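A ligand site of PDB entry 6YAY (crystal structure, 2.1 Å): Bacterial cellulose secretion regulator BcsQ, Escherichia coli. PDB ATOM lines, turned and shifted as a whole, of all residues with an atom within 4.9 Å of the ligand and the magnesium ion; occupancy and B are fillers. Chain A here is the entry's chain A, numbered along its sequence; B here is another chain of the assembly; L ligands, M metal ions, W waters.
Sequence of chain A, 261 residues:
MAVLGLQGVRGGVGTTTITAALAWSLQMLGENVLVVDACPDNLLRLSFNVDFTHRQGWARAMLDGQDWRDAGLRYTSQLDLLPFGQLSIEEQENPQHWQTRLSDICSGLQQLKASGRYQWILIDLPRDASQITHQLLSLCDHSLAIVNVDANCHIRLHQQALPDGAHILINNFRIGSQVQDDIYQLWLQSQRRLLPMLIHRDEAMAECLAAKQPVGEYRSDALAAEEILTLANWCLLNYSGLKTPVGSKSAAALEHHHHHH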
ATOM      1  N   ARG A  10      17.447   6.182  18.228  1.00  0.00           N
ATOM      2  CA  ARG A  10      16.400   6.137  19.250  1.00  0.00           C
ATOM      3  C   ARG A  10      15.180   6.867  18.692  1.00  0.00           C
ATOM      4  O   ARG A  10      15.205   7.405  17.593  1.00  0.00           O
ATOM      5  CB  ARG A  10      16.883   6.759  20.567  1.00  0.00           C
ATOM      6  CG  ARG A  10      17.045   8.251  20.516  1.00  0.00           C
ATOM      7  CD  ARG A  10      16.903   8.878  21.897  1.00  0.00           C
ATOM      8  NE  ARG A  10      16.919  10.335  21.817  1.00  0.00           N
ATOM      9  CZ  ARG A  10      18.017  11.067  21.967  1.00  0.00           C
ATOM     10  NH1 ARG A  10      19.185  10.486  22.215  1.00  0.00           N
ATOM     11  NH2 ARG A  10      17.946  12.387  21.881  1.00  0.00           N
ATOM     12  N   GLY A  11      14.108   6.873  19.480  1.00  0.00           N
ATOM     13  CA  GLY A  11      12.905   7.570  19.055  1.00  0.00           C
ATOM     14  C   GLY A  11      13.058   9.074  19.161  1.00  0.00           C
ATOM     15  O   GLY A  11      13.841   9.601  19.943  1.00  0.00           O
ATOM     16  N   GLY A  12      12.281   9.784  18.333  1.00  0.00           N
ATOM     17  CA  GLY A  12      12.181  11.226  18.400  1.00  0.00           C
ATOM     18  C   GLY A  12      13.367  12.009  17.897  1.00  0.00           C
ATOM     19  O   GLY A  12      13.445  13.215  18.176  1.00  0.00           O
ATOM     20  N   VAL A  13      14.285  11.397  17.153  1.00  0.00           N
ATOM     21  CA  VAL A  13      15.463  12.119  16.648  1.00  0.00           C
ATOM     22  C   VAL A  13      15.184  12.857  15.347  1.00  0.00           C
ATOM     23  O   VAL A  13      16.039  13.653  14.914  1.00  0.00           O
ATOM     24  CB  VAL A  13      16.651  11.161  16.439  1.00  0.00           C
ATOM     25  CG1 VAL A  13      17.185  10.680  17.780  1.00  0.00           C
ATOM     26  CG2 VAL A  13      16.254   9.992  15.556  1.00  0.00           C
ATOM     27  N   GLY A  14      14.039  12.640  14.707  1.00  0.00           N
ATOM     28  CA  GLY A  14      13.685  13.355  13.497  1.00  0.00           C
ATOM     29  C   GLY A  14      13.576  12.470  12.272  1.00  0.00           C
ATOM     30  O   GLY A  14      13.621  12.958  11.140  1.00  0.00           O
ATOM     31  N   THR A  15      13.419  11.168  12.495  1.00  0.00           N
ATOM     32  CA  THR A  15      13.462  10.195  11.405  1.00  0.00           C
ATOM     33  C   THR A  15      12.356  10.445  10.386  1.00  0.00           C
ATOM     34  O   THR A  15      12.603  10.461   9.181  1.00  0.00           O
ATOM     35  CB  THR A  15      13.365   8.776  11.969  1.00  0.00           C
ATOM     36  OG1 THR A  15      14.358   8.584  12.978  1.00  0.00           O
ATOM     37  CG2 THR A  15      13.590   7.755  10.868  1.00  0.00           C
ATOM     38  N   THR A  16      11.131  10.642  10.867  1.00  0.00           N
ATOM     39  CA  THR A  16       9.994  10.790   9.959  1.00  0.00           C
ATOM     40  C   THR A  16      10.051  12.101   9.192  1.00  0.00           C
ATOM     41  O   THR A  16       9.758  12.137   7.986  1.00  0.00           O
ATOM     42  CB  THR A  16       8.689  10.676  10.753  1.00  0.00           C
ATOM     43  OG1 THR A  16       8.592   9.372  11.323  1.00  0.00           O
ATOM     44  CG2 THR A  16       7.486  10.927   9.855  1.00  0.00           C
ATOM     45  N   THR A  17      10.447  13.181   9.857  1.00  0.00           N
ATOM     46  CA  THR A  17      10.527  14.483   9.189  1.00  0.00           C
ATOM     47  C   THR A  17      11.600  14.471   8.107  1.00  0.00           C
ATOM     48  O   THR A  17      11.398  15.015   7.021  1.00  0.00           O
ATOM     49  CB  THR A  17      10.796  15.579  10.205  1.00  0.00           C
ATOM     50  OG1 THR A  17       9.859  15.471  11.284  1.00  0.00           O
ATOM     51  CG2 THR A  17      10.640  16.949   9.567  1.00  0.00           C
ATOM     52  N   ILE A  18      12.739  13.829   8.384  1.00  0.00           N
ATOM     53  CA  ILE A  18      13.807  13.759   7.395  1.00  0.00           C
ATOM     54  C   ILE A  18      13.386  12.894   6.219  1.00  0.00           C
ATOM     55  O   ILE A  18      13.707  13.199   5.060  1.00  0.00           O
ATOM     56  CB  ILE A  18      15.097  13.231   8.050  1.00  0.00           C
ATOM     57  CG1 ILE A  18      15.638  14.250   9.067  1.00  0.00           C
ATOM     58  CG2 ILE A  18      16.143  12.892   7.003  1.00  0.00           C
ATOM     59  CD1 ILE A  18      16.851  13.763   9.819  1.00  0.00           C
ATOM     60  N   CYS A  39       6.182   2.515  10.344  1.00  0.00           N
ATOM     61  CA  CYS A  39       5.970   2.782  11.756  1.00  0.00           C
ATOM     62  C   CYS A  39       4.488   2.654  12.097  1.00  0.00           C
ATOM     63  O   CYS A  39       3.655   3.278  11.434  1.00  0.00           O
ATOM     64  CB  CYS A  39       6.453   4.178  12.116  1.00  0.00           C
ATOM     65  SG  CYS A  39       8.222   4.413  11.833  1.00  0.00           S
ATOM     66  N   ASP A  41       2.922   4.017  14.345  1.00  0.00           N
ATOM     67  CA  ASP A  41       2.406   5.340  14.683  1.00  0.00           C
ATOM     68  C   ASP A  41       1.686   5.978  13.495  1.00  0.00           C
ATOM     69  O   ASP A  41       0.801   6.810  13.692  1.00  0.00           O
ATOM     70  CB  ASP A  41       3.547   6.241  15.143  1.00  0.00           C
ATOM     71  CG  ASP A  41       4.541   5.519  16.038  1.00  0.00           C
ATOM     72  OD1 ASP A  41       4.114   4.922  17.052  1.00  0.00           O
ATOM     73  OD2 ASP A  41       5.751   5.558  15.719  1.00  0.00           O
ATOM     74  N   LEU A  43       2.597   8.148  11.211  1.00  0.00           N
ATOM     75  CA  LEU A  43       2.744   9.595  11.269  1.00  0.00           C
ATOM     76  C   LEU A  43       3.242  10.217   9.969  1.00  0.00           C
ATOM     77  O   LEU A  43       3.016  11.406   9.746  1.00  0.00           O
ATOM     78  CB  LEU A  43       3.715   9.979  12.399  1.00  0.00           C
ATOM     79  CG  LEU A  43       3.249   9.613  13.812  1.00  0.00           C
ATOM     80  CD1 LEU A  43       4.303   9.968  14.847  1.00  0.00           C
ATOM     81  CD2 LEU A  43       1.936  10.303  14.119  1.00  0.00           C
ATOM     82  N   ASP A 124      10.419   4.586   6.119  1.00  0.00           N
ATOM     83  CA  ASP A 124      10.504   5.123   7.474  1.00  0.00           C
ATOM     84  C   ASP A 124      10.358   3.956   8.447  1.00  0.00           C
ATOM     85  O   ASP A 124       9.270   3.410   8.623  1.00  0.00           O
ATOM     86  CB  ASP A 124       9.424   6.182   7.692  1.00  0.00           C
ATOM     87  CG  ASP A 124       9.451   6.781   9.089  1.00  0.00           C
ATOM     88  OD1 ASP A 124      10.414   6.547   9.851  1.00  0.00           O
ATOM     89  OD2 ASP A 124       8.492   7.507   9.437  1.00  0.00           O
ATOM     90  N   ASN A 171      20.959  15.025  13.188  1.00  0.00           N
ATOM     91  CA  ASN A 171      19.830  15.940  13.061  1.00  0.00           C
ATOM     92  C   ASN A 171      19.740  16.807  14.306  1.00  0.00           C
ATOM     93  O   ASN A 171      20.306  16.474  15.353  1.00  0.00           O
ATOM     94  CB  ASN A 171      18.514  15.171  12.844  1.00  0.00           C
ATOM     95  CG  ASN A 171      17.340  16.095  12.579  1.00  0.00           C
ATOM     96  OD1 ASN A 171      17.453  17.094  11.869  1.00  0.00           O
ATOM     97  ND2 ASN A 171      16.187  15.768  13.167  1.00  0.00           N
ATOM     98  N   ASN A 172      19.047  17.936  14.178  1.00  0.00           N
ATOM     99  CA  ASN A 172      18.736  18.815  15.303  1.00  0.00           C
ATOM    100  C   ASN A 172      19.998  19.419  15.926  1.00  0.00           C
ATOM    101  O   ASN A 172      20.008  19.783  17.101  1.00  0.00           O
ATOM    102  CB  ASN A 172      17.933  18.076  16.383  1.00  0.00           C
ATOM    103  CG  ASN A 172      16.503  18.573  16.471  1.00  0.00           C
ATOM    104  OD1 ASN A 172      16.253  19.773  16.402  1.00  0.00           O
ATOM    105  ND2 ASN A 172      15.569  17.642  16.636  1.00  0.00           N
ATOM    106  N   ILE A 199      22.006  18.091   9.710  1.00  0.00           N
ATOM    107  CA  ILE A 199      20.819  18.940   9.654  1.00  0.00           C
ATOM    108  C   ILE A 199      20.745  19.733  10.955  1.00  0.00           C
ATOM    109  O   ILE A 199      20.595  19.149  12.030  1.00  0.00           O
ATOM    110  CB  ILE A 199      19.541  18.106   9.456  1.00  0.00           C
ATOM    111  CG1 ILE A 199      19.756  17.019   8.400  1.00  0.00           C
ATOM    112  CG2 ILE A 199      18.374  19.014   9.080  1.00  0.00           C
ATOM    113  CD1 ILE A 199      20.137  17.537   7.030  1.00  0.00           C
ATOM    114  N   HIS A 200      20.870  21.055  10.861  1.00  0.00           N
ATOM    115  CA  HIS A 200      20.731  21.911  12.025  1.00  0.00           C
ATOM    116  C   HIS A 200      19.293  21.899  12.546  1.00  0.00           C
ATOM    117  O   HIS A 200      18.341  21.631  11.802  1.00  0.00           O
ATOM    118  CB  HIS A 200      21.125  23.357  11.708  1.00  0.00           C
ATOM    119  CG  HIS A 200      22.594  23.579  11.554  1.00  0.00           C
ATOM    120  ND1 HIS A 200      23.286  23.262  10.407  1.00  0.00           N
ATOM    121  CD2 HIS A 200      23.512  24.092  12.415  1.00  0.00           C
ATOM    122  CE1 HIS A 200      24.557  23.570  10.566  1.00  0.00           C
ATOM    123  NE2 HIS A 200      24.721  24.079  11.772  1.00  0.00           N
ATOM    124  N   ARG A 201      19.144  22.203  13.830  1.00  0.00           N
ATOM    125  CA  ARG A 201      17.816  22.517  14.332  1.00  0.00           C
ATOM    126  C   ARG A 201      17.270  23.717  13.575  1.00  0.00           C
ATOM    127  O   ARG A 201      18.000  24.660  13.276  1.00  0.00           O
ATOM    128  CB  ARG A 201      17.845  22.813  15.840  1.00  0.00           C
ATOM    129  CG  ARG A 201      16.463  23.073  16.432  1.00  0.00           C
ATOM    130  CD  ARG A 201      16.489  23.407  17.922  1.00  0.00           C
ATOM    131  NE  ARG A 201      16.738  22.230  18.756  1.00  0.00           N
ATOM    132  CZ  ARG A 201      15.797  21.355  19.107  1.00  0.00           C
ATOM    133  NH1 ARG A 201      14.550  21.509  18.683  1.00  0.00           N
ATOM    134  NH2 ARG A 201      16.121  20.325  19.868  1.00  0.00           N
ATOM    135  N   ASP A 202      15.984  23.683  13.260  1.00  0.00           N
ATOM    136  CA  ASP A 202      15.373  24.701  12.418  1.00  0.00           C
ATOM    137  C   ASP A 202      13.890  24.728  12.701  1.00  0.00           C
ATOM    138  O   ASP A 202      13.232  23.680  12.631  1.00  0.00           O
ATOM    139  CB  ASP A 202      15.648  24.405  10.941  1.00  0.00           C
ATOM    140  CG  ASP A 202      15.313  25.566  10.031  1.00  0.00           C
ATOM    141  OD1 ASP A 202      14.339  26.293  10.305  1.00  0.00           O
ATOM    142  OD2 ASP A 202      16.034  25.759   9.027  1.00  0.00           O
ATOM    143  N   MET A 205      11.635  22.891  10.451  1.00  0.00           N
ATOM    144  CA  MET A 205      11.480  21.462  10.686  1.00  0.00           C
ATOM    145  C   MET A 205      10.429  21.176  11.747  1.00  0.00           C
ATOM    146  O   MET A 205       9.800  20.111  11.748  1.00  0.00           O
ATOM    147  CB  MET A 205      12.814  20.845  11.113  1.00  0.00           C
ATOM    148  CG  MET A 205      13.872  20.809  10.029  1.00  0.00           C
ATOM    149  SD  MET A 205      13.657  19.342   8.750  1.00  0.00           S
ATOM    150  CE  MET A 205      14.145  17.846   9.919  1.00  0.00           C
ATOM    151  N   ALA A 206      10.240  22.125  12.661  1.00  0.00           N
ATOM    152  CA  ALA A 206       9.193  21.973  13.671  1.00  0.00           C
ATOM    153  C   ALA A 206       7.838  22.399  13.156  1.00  0.00           C
ATOM    154  O   ALA A 206       6.810  21.839  13.573  1.00  0.00           O
ATOM    155  CB  ALA A 206       9.560  22.761  14.935  1.00  0.00           C
ATOM    156  N   LEU A 209       5.504  19.982   9.882  1.00  0.00           N
ATOM    157  CA  LEU A 209       4.518  18.964  10.265  1.00  0.00           C
ATOM    158  C   LEU A 209       3.211  19.599  10.725  1.00  0.00           C
ATOM    159  O   LEU A 209       2.122  19.085  10.431  1.00  0.00           O
ATOM    160  CB  LEU A 209       5.088  18.063  11.358  1.00  0.00           C
ATOM    161  CG  LEU A 209       4.199  16.921  11.831  1.00  0.00           C
ATOM    162  CD1 LEU A 209       3.785  16.052  10.651  1.00  0.00           C
ATOM    163  CD2 LEU A 209       4.905  16.076  12.892  1.00  0.00           C
ATOM    164  N   ARG B  10       6.560   9.153  23.422  1.00  0.00           N
ATOM    165  CA  ARG B  10       7.460   8.616  22.409  1.00  0.00           C
ATOM    166  C   ARG B  10       8.852   8.528  23.015  1.00  0.00           C
ATOM    167  O   ARG B  10       9.081   8.975  24.146  1.00  0.00           O
ATOM    168  CB  ARG B  10       7.473   9.477  21.138  1.00  0.00           C
ATOM    169  CG  ARG B  10       8.176  10.797  21.329  1.00  0.00           C
ATOM    170  CD  ARG B  10       8.842  11.270  20.044  1.00  0.00           C
ATOM    171  NE  ARG B  10       9.658  12.449  20.305  1.00  0.00           N
ATOM    172  CZ  ARG B  10       9.207  13.693  20.237  1.00  0.00           C
ATOM    173  NH1 ARG B  10       7.937  13.920  19.933  1.00  0.00           N
ATOM    174  NH2 ARG B  10      10.017  14.705  20.484  1.00  0.00           N
ATOM    175  N   GLY B  11       9.786   7.956  22.263  1.00  0.00           N
ATOM    176  CA  GLY B  11      11.146   7.861  22.745  1.00  0.00           C
ATOM    177  C   GLY B  11      11.876   9.190  22.724  1.00  0.00           C
ATOM    178  O   GLY B  11      11.546  10.114  21.985  1.00  0.00           O
ATOM    179  N   ASP B 150       5.514  19.456  20.825  1.00  0.00           N
ATOM    180  CA  ASP B 150       5.757  19.535  19.390  1.00  0.00           C
ATOM    181  C   ASP B 150       4.622  18.828  18.661  1.00  0.00           C
ATOM    182  O   ASP B 150       3.762  18.195  19.277  1.00  0.00           O
ATOM    183  CB  ASP B 150       7.126  18.943  19.024  1.00  0.00           C
ATOM    184  CG  ASP B 150       7.294  17.496  19.482  1.00  0.00           C
ATOM    185  OD1 ASP B 150       6.296  16.770  19.628  1.00  0.00           O
ATOM    186  OD2 ASP B 150       8.463  17.091  19.701  1.00  0.00           O
ATOM    187  N   ALA B 151       4.621  18.955  17.331  1.00  0.00           N
ATOM    188  CA  ALA B 151       3.538  18.391  16.537  1.00  0.00           C
ATOM    189  C   ALA B 151       3.467  16.868  16.671  1.00  0.00           C
ATOM    190  O   ALA B 151       2.376  16.291  16.640  1.00  0.00           O
ATOM    191  CB  ALA B 151       3.697  18.794  15.075  1.00  0.00           C
ATOM    192  N   ASN B 152       4.617  16.210  16.821  1.00  0.00           N
ATOM    193  CA  ASN B 152       4.638  14.756  16.967  1.00  0.00           C
ATOM    194  C   ASN B 152       3.848  14.322  18.192  1.00  0.00           C
ATOM    195  O   ASN B 152       2.900  13.531  18.077  1.00  0.00           O
ATOM    196  CB  ASN B 152       6.099  14.278  17.055  1.00  0.00           C
ATOM    197  CG  ASN B 152       6.228  12.757  17.164  1.00  0.00           C
ATOM    198  OD1 ASN B 152       5.513  12.112  17.920  1.00  0.00           O
ATOM    199  ND2 ASN B 152       7.168  12.189  16.419  1.00  0.00           N
ATOM    200  N   ARG B 156       0.171  12.238  18.760  1.00  0.00           N
ATOM    201  CA  ARG B 156       0.098  10.972  19.501  1.00  0.00           C
ATOM    202  C   ARG B 156      -0.949  11.033  20.606  1.00  0.00           C
ATOM    203  O   ARG B 156      -1.598  10.019  20.891  1.00  0.00           O
ATOM    204  CB  ARG B 156       1.470  10.627  20.084  1.00  0.00           C
ATOM    205  CG  ARG B 156       2.495  10.175  19.062  1.00  0.00           C
ATOM    206  CD  ARG B 156       3.865   9.980  19.704  1.00  0.00           C
ATOM    207  NE  ARG B 156       4.849   9.450  18.774  1.00  0.00           N
ATOM    208  CZ  ARG B 156       5.083   8.150  18.586  1.00  0.00           C
ATOM    209  NH1 ARG B 156       4.386   7.257  19.269  1.00  0.00           N
ATOM    210  NH2 ARG B 156       6.004   7.754  17.732  1.00  0.00           N
HETATM  211  P1  LIG L   1       9.157   8.940  16.432  1.00  0.00           P
HETATM  212  O1  LIG L   1       9.981   8.208  17.417  1.00  0.00           O
HETATM  213  O2  LIG L   1       8.925   8.167  15.147  1.00  0.00           O
HETATM  214  O3  LIG L   1       7.781   9.344  16.966  1.00  0.00           O
HETATM  215  P2  LIG L   1      10.947  10.624  14.880  1.00  0.00           P
HETATM  216  O4  LIG L   1      12.316  10.142  15.174  1.00  0.00           O
HETATM  217  O5  LIG L   1      10.324  10.122  13.583  1.00  0.00           O
HETATM  218  O6  LIG L   1       9.899  10.300  16.030  1.00  0.00           O
HETATM  219  P3  LIG L   1      10.005  13.263  14.084  1.00  0.00           P
HETATM  220  O7  LIG L   1       8.582  12.935  14.218  1.00  0.00           O
HETATM  221  O8  LIG L   1      10.557  13.375  12.658  1.00  0.00           O
HETATM  222  O9  LIG L   1      10.913  12.205  14.843  1.00  0.00           O
HETATM  223  O10 LIG L   1      10.391  14.600  14.854  1.00  0.00           O
HETATM  224  C1  LIG L   1      10.013  14.781  16.228  1.00  0.00           C
HETATM  225  C2  LIG L   1       9.713  16.237  16.468  1.00  0.00           C
HETATM  226  O11 LIG L   1      10.924  17.009  16.346  1.00  0.00           O
HETATM  227  C3  LIG L   1       8.704  16.861  15.498  1.00  0.00           C
HETATM  228  O12 LIG L   1       7.842  17.779  16.166  1.00  0.00           O
HETATM  229  C4  LIG L   1       9.602  17.578  14.478  1.00  0.00           C
HETATM  230  O13 LIG L   1       8.956  18.693  13.895  1.00  0.00           O
HETATM  231  C5  LIG L   1      10.775  18.013  15.355  1.00  0.00           C
HETATM  232  N1  LIG L   1      12.043  18.115  14.642  1.00  0.00           N
HETATM  233  C6  LIG L   1      12.659  17.135  13.901  1.00  0.00           C
HETATM  234  N2  LIG L   1      13.784  17.499  13.343  1.00  0.00           N
HETATM  235  C7  LIG L   1      13.927  18.825  13.741  1.00  0.00           C
HETATM  236  C8  LIG L   1      14.915  19.785  13.487  1.00  0.00           C
HETATM  237  N3  LIG L   1      16.005  19.559  12.738  1.00  0.00           N
HETATM  238  N4  LIG L   1      14.752  21.017  14.036  1.00  0.00           N
HETATM  239  C9  LIG L   1      13.677  21.252  14.783  1.00  0.00           C
HETATM  240  N5  LIG L   1      12.673  20.418  15.093  1.00  0.00           N
HETATM  241  C10 LIG L   1      12.859  19.215  14.537  1.00  0.00           C
HETATM  242 MG    MG M   1       8.761   8.623  13.173  1.00  0.00          MG
HETATM  243  O   HOH W   1       7.610  10.167  13.674  1.00  0.00           O
HETATM  244  O   HOH W   2       6.957   7.355  12.975  1.00  0.00           O
HETATM  245  O   HOH W   3      10.415   7.065  12.460  1.00  0.00           O
HETATM  246  O   HOH W   4       9.417   6.762  19.460  1.00  0.00           O
HETATM  247  O   HOH W   5       6.914  20.622  16.080  1.00  0.00           O
HETATM  248  O   HOH W   6      13.532   7.847  15.196  1.00  0.00           O
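N of Asn 152 of chain B sits close to OD1 of Asp 150 of chain B, 3.3 Å away.
OD2 of Asp 124 lies close to OG1 of Thr 16.
NH2 of Arg 10 of chain B is in salt-bridge range of OD2 of Asp 150 of chain B.
OD1 of Asn 172 sits close to NH1 of Arg 201 (3.3 Å).
The guanidinium group of Arg 156 of chain B sits at hydrogen-bond distance from the side-chain amide oxygen of Asn 152 of chain B.
The backbone carbonyl oxygen of Val 13 lies within hydrogen-bond range of the side-chain amide nitrogen of Asn 171 (2.7 Å).
OD2 of Asp 41 is in salt-bridge range of NH2 of Arg 156 of chain B (3.0 Å).
The side-chain sulfur of Cys 39 is in hydrogen-bond range of the backbone carbonyl oxygen of Asp 124 (3.5 Å).
The magnesium ion is bound by water W1, OG1 of Thr 16, O2 of the ligand, O5 of the ligand, water W2 and water W3.
The magnesium ion has six donor atoms within binding distance.
Water W1 lies within hydrogen-bond range of O7 of the ligand (3.0 Å) and ND2 of Asn 152 of chain B (3.4 Å).
Water W3 lies within hydrogen-bond range of the side-chain carboxylate of Asp 124 (2.7 Å) and the side-chain sulfur of Cys 39 (3.5 Å).
Water W2 lies within hydrogen-bond range of the side-chain sulfur of Cys 39 (3.4 Å) and the side-chain carboxylate of Asp 41 (3.5 Å).
Water W4 lies within hydrogen-bond range of an oxygen (O1) of the ligand and the backbone NH (N) of Gly 11 of chain B.
Water W6 lies within hydrogen-bond range of OG1 of Thr 15 (2.5 Å), O4 of the ligand (2.6 Å) and O of Arg 10 of chain A (3.0 Å).
Water W5 lies within hydrogen-bond range of the backbone carbonyl oxygen of Ala 206, an oxygen (O12) of the ligand and the backbone NH of Ala 151 of chain B.
The backbone NH (N) of Thr 17 is in hydrogen-bond range of an oxygen (O8) of the ligand.
An oxygen (O4) of the ligand is in hydrogen-bond range of the backbone NH (N) of Val 13 (3.1 Å).
The backbone NH (N) of Gly 14 sits at hydrogen-bond distance from an oxygen (O4) of the ligand, 3.1 Å away.
An oxygen (O3) of the ligand is in salt-bridge range of the guanidinium group (NH2) of Arg 156 of chain B (2.5 Å).
N of Asp 202 sits at hydrogen-bond distance from N4 of the ligand (3.0 Å).
The side-chain hydroxyl of Thr 17 is in hydrogen-bond range of an oxygen (O8) of the ligand.
O of Met 205 sits at hydrogen-bond distance from O13 of the ligand (2.7 Å).
An oxygen (O8) of the ligand is in hydrogen-bond range of the backbone NH of Thr 16 (3.3 Å).
A nitrogen (N4) of the ligand lies close to the side-chain amide oxygen of Asn 172 (3.1 Å).
The backbone NH of Thr 15 sits at hydrogen-bond distance from an oxygen (O4) of the ligand (3.1 Å).
The side-chain hydroxyl (OG1) of Thr 15 sits at hydrogen-bond distance from an oxygen (O4) of the ligand (3.4 Å).
N2 of the ligand sits at hydrogen-bond distance from ND2 of Asn 171, at 3.0 Å.
The side-chain amide nitrogen (ND2) of Asn 152 of chain B lies within hydrogen-bond range of an oxygen (O7) of the ligand (2.7 Å).
A nitrogen (N3) of the ligand sits at hydrogen-bond distance from the backbone carbonyl oxygen (O) of His 200 (3.3 Å).
O1 of the ligand sits at hydrogen-bond distance from N of Gly 12 (2.9 Å).
Gly 11 of chain A touches the ligand.
Arg 201 touches the ligand (CA to N4, 3.4 Å).
Ala 206 touches the ligand.
Arg 10 of chain B touches the ligand.
CB of Asp 150 of chain B touches O12 of the ligand (3.2 Å).
N of Ala 151 of chain B touches O12 of the ligand, at 3.6 Å.
Hydrophobic or aromatic side chains within 4 Å of the ligand: Val 13, Met 205 and Ala 206.
The nearest printed residue that does not touch the ligand is Leu 43 (4.1 Å).
Asp 124 touches the magnesium ion (OD2 to MG, 3.9 Å).
Within 4 Å of the magnesium ion: Thr 16 and Asp 124.
The nearest printed residue that does not touch the magnesium ion is Cys 39 (4.5 Å).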
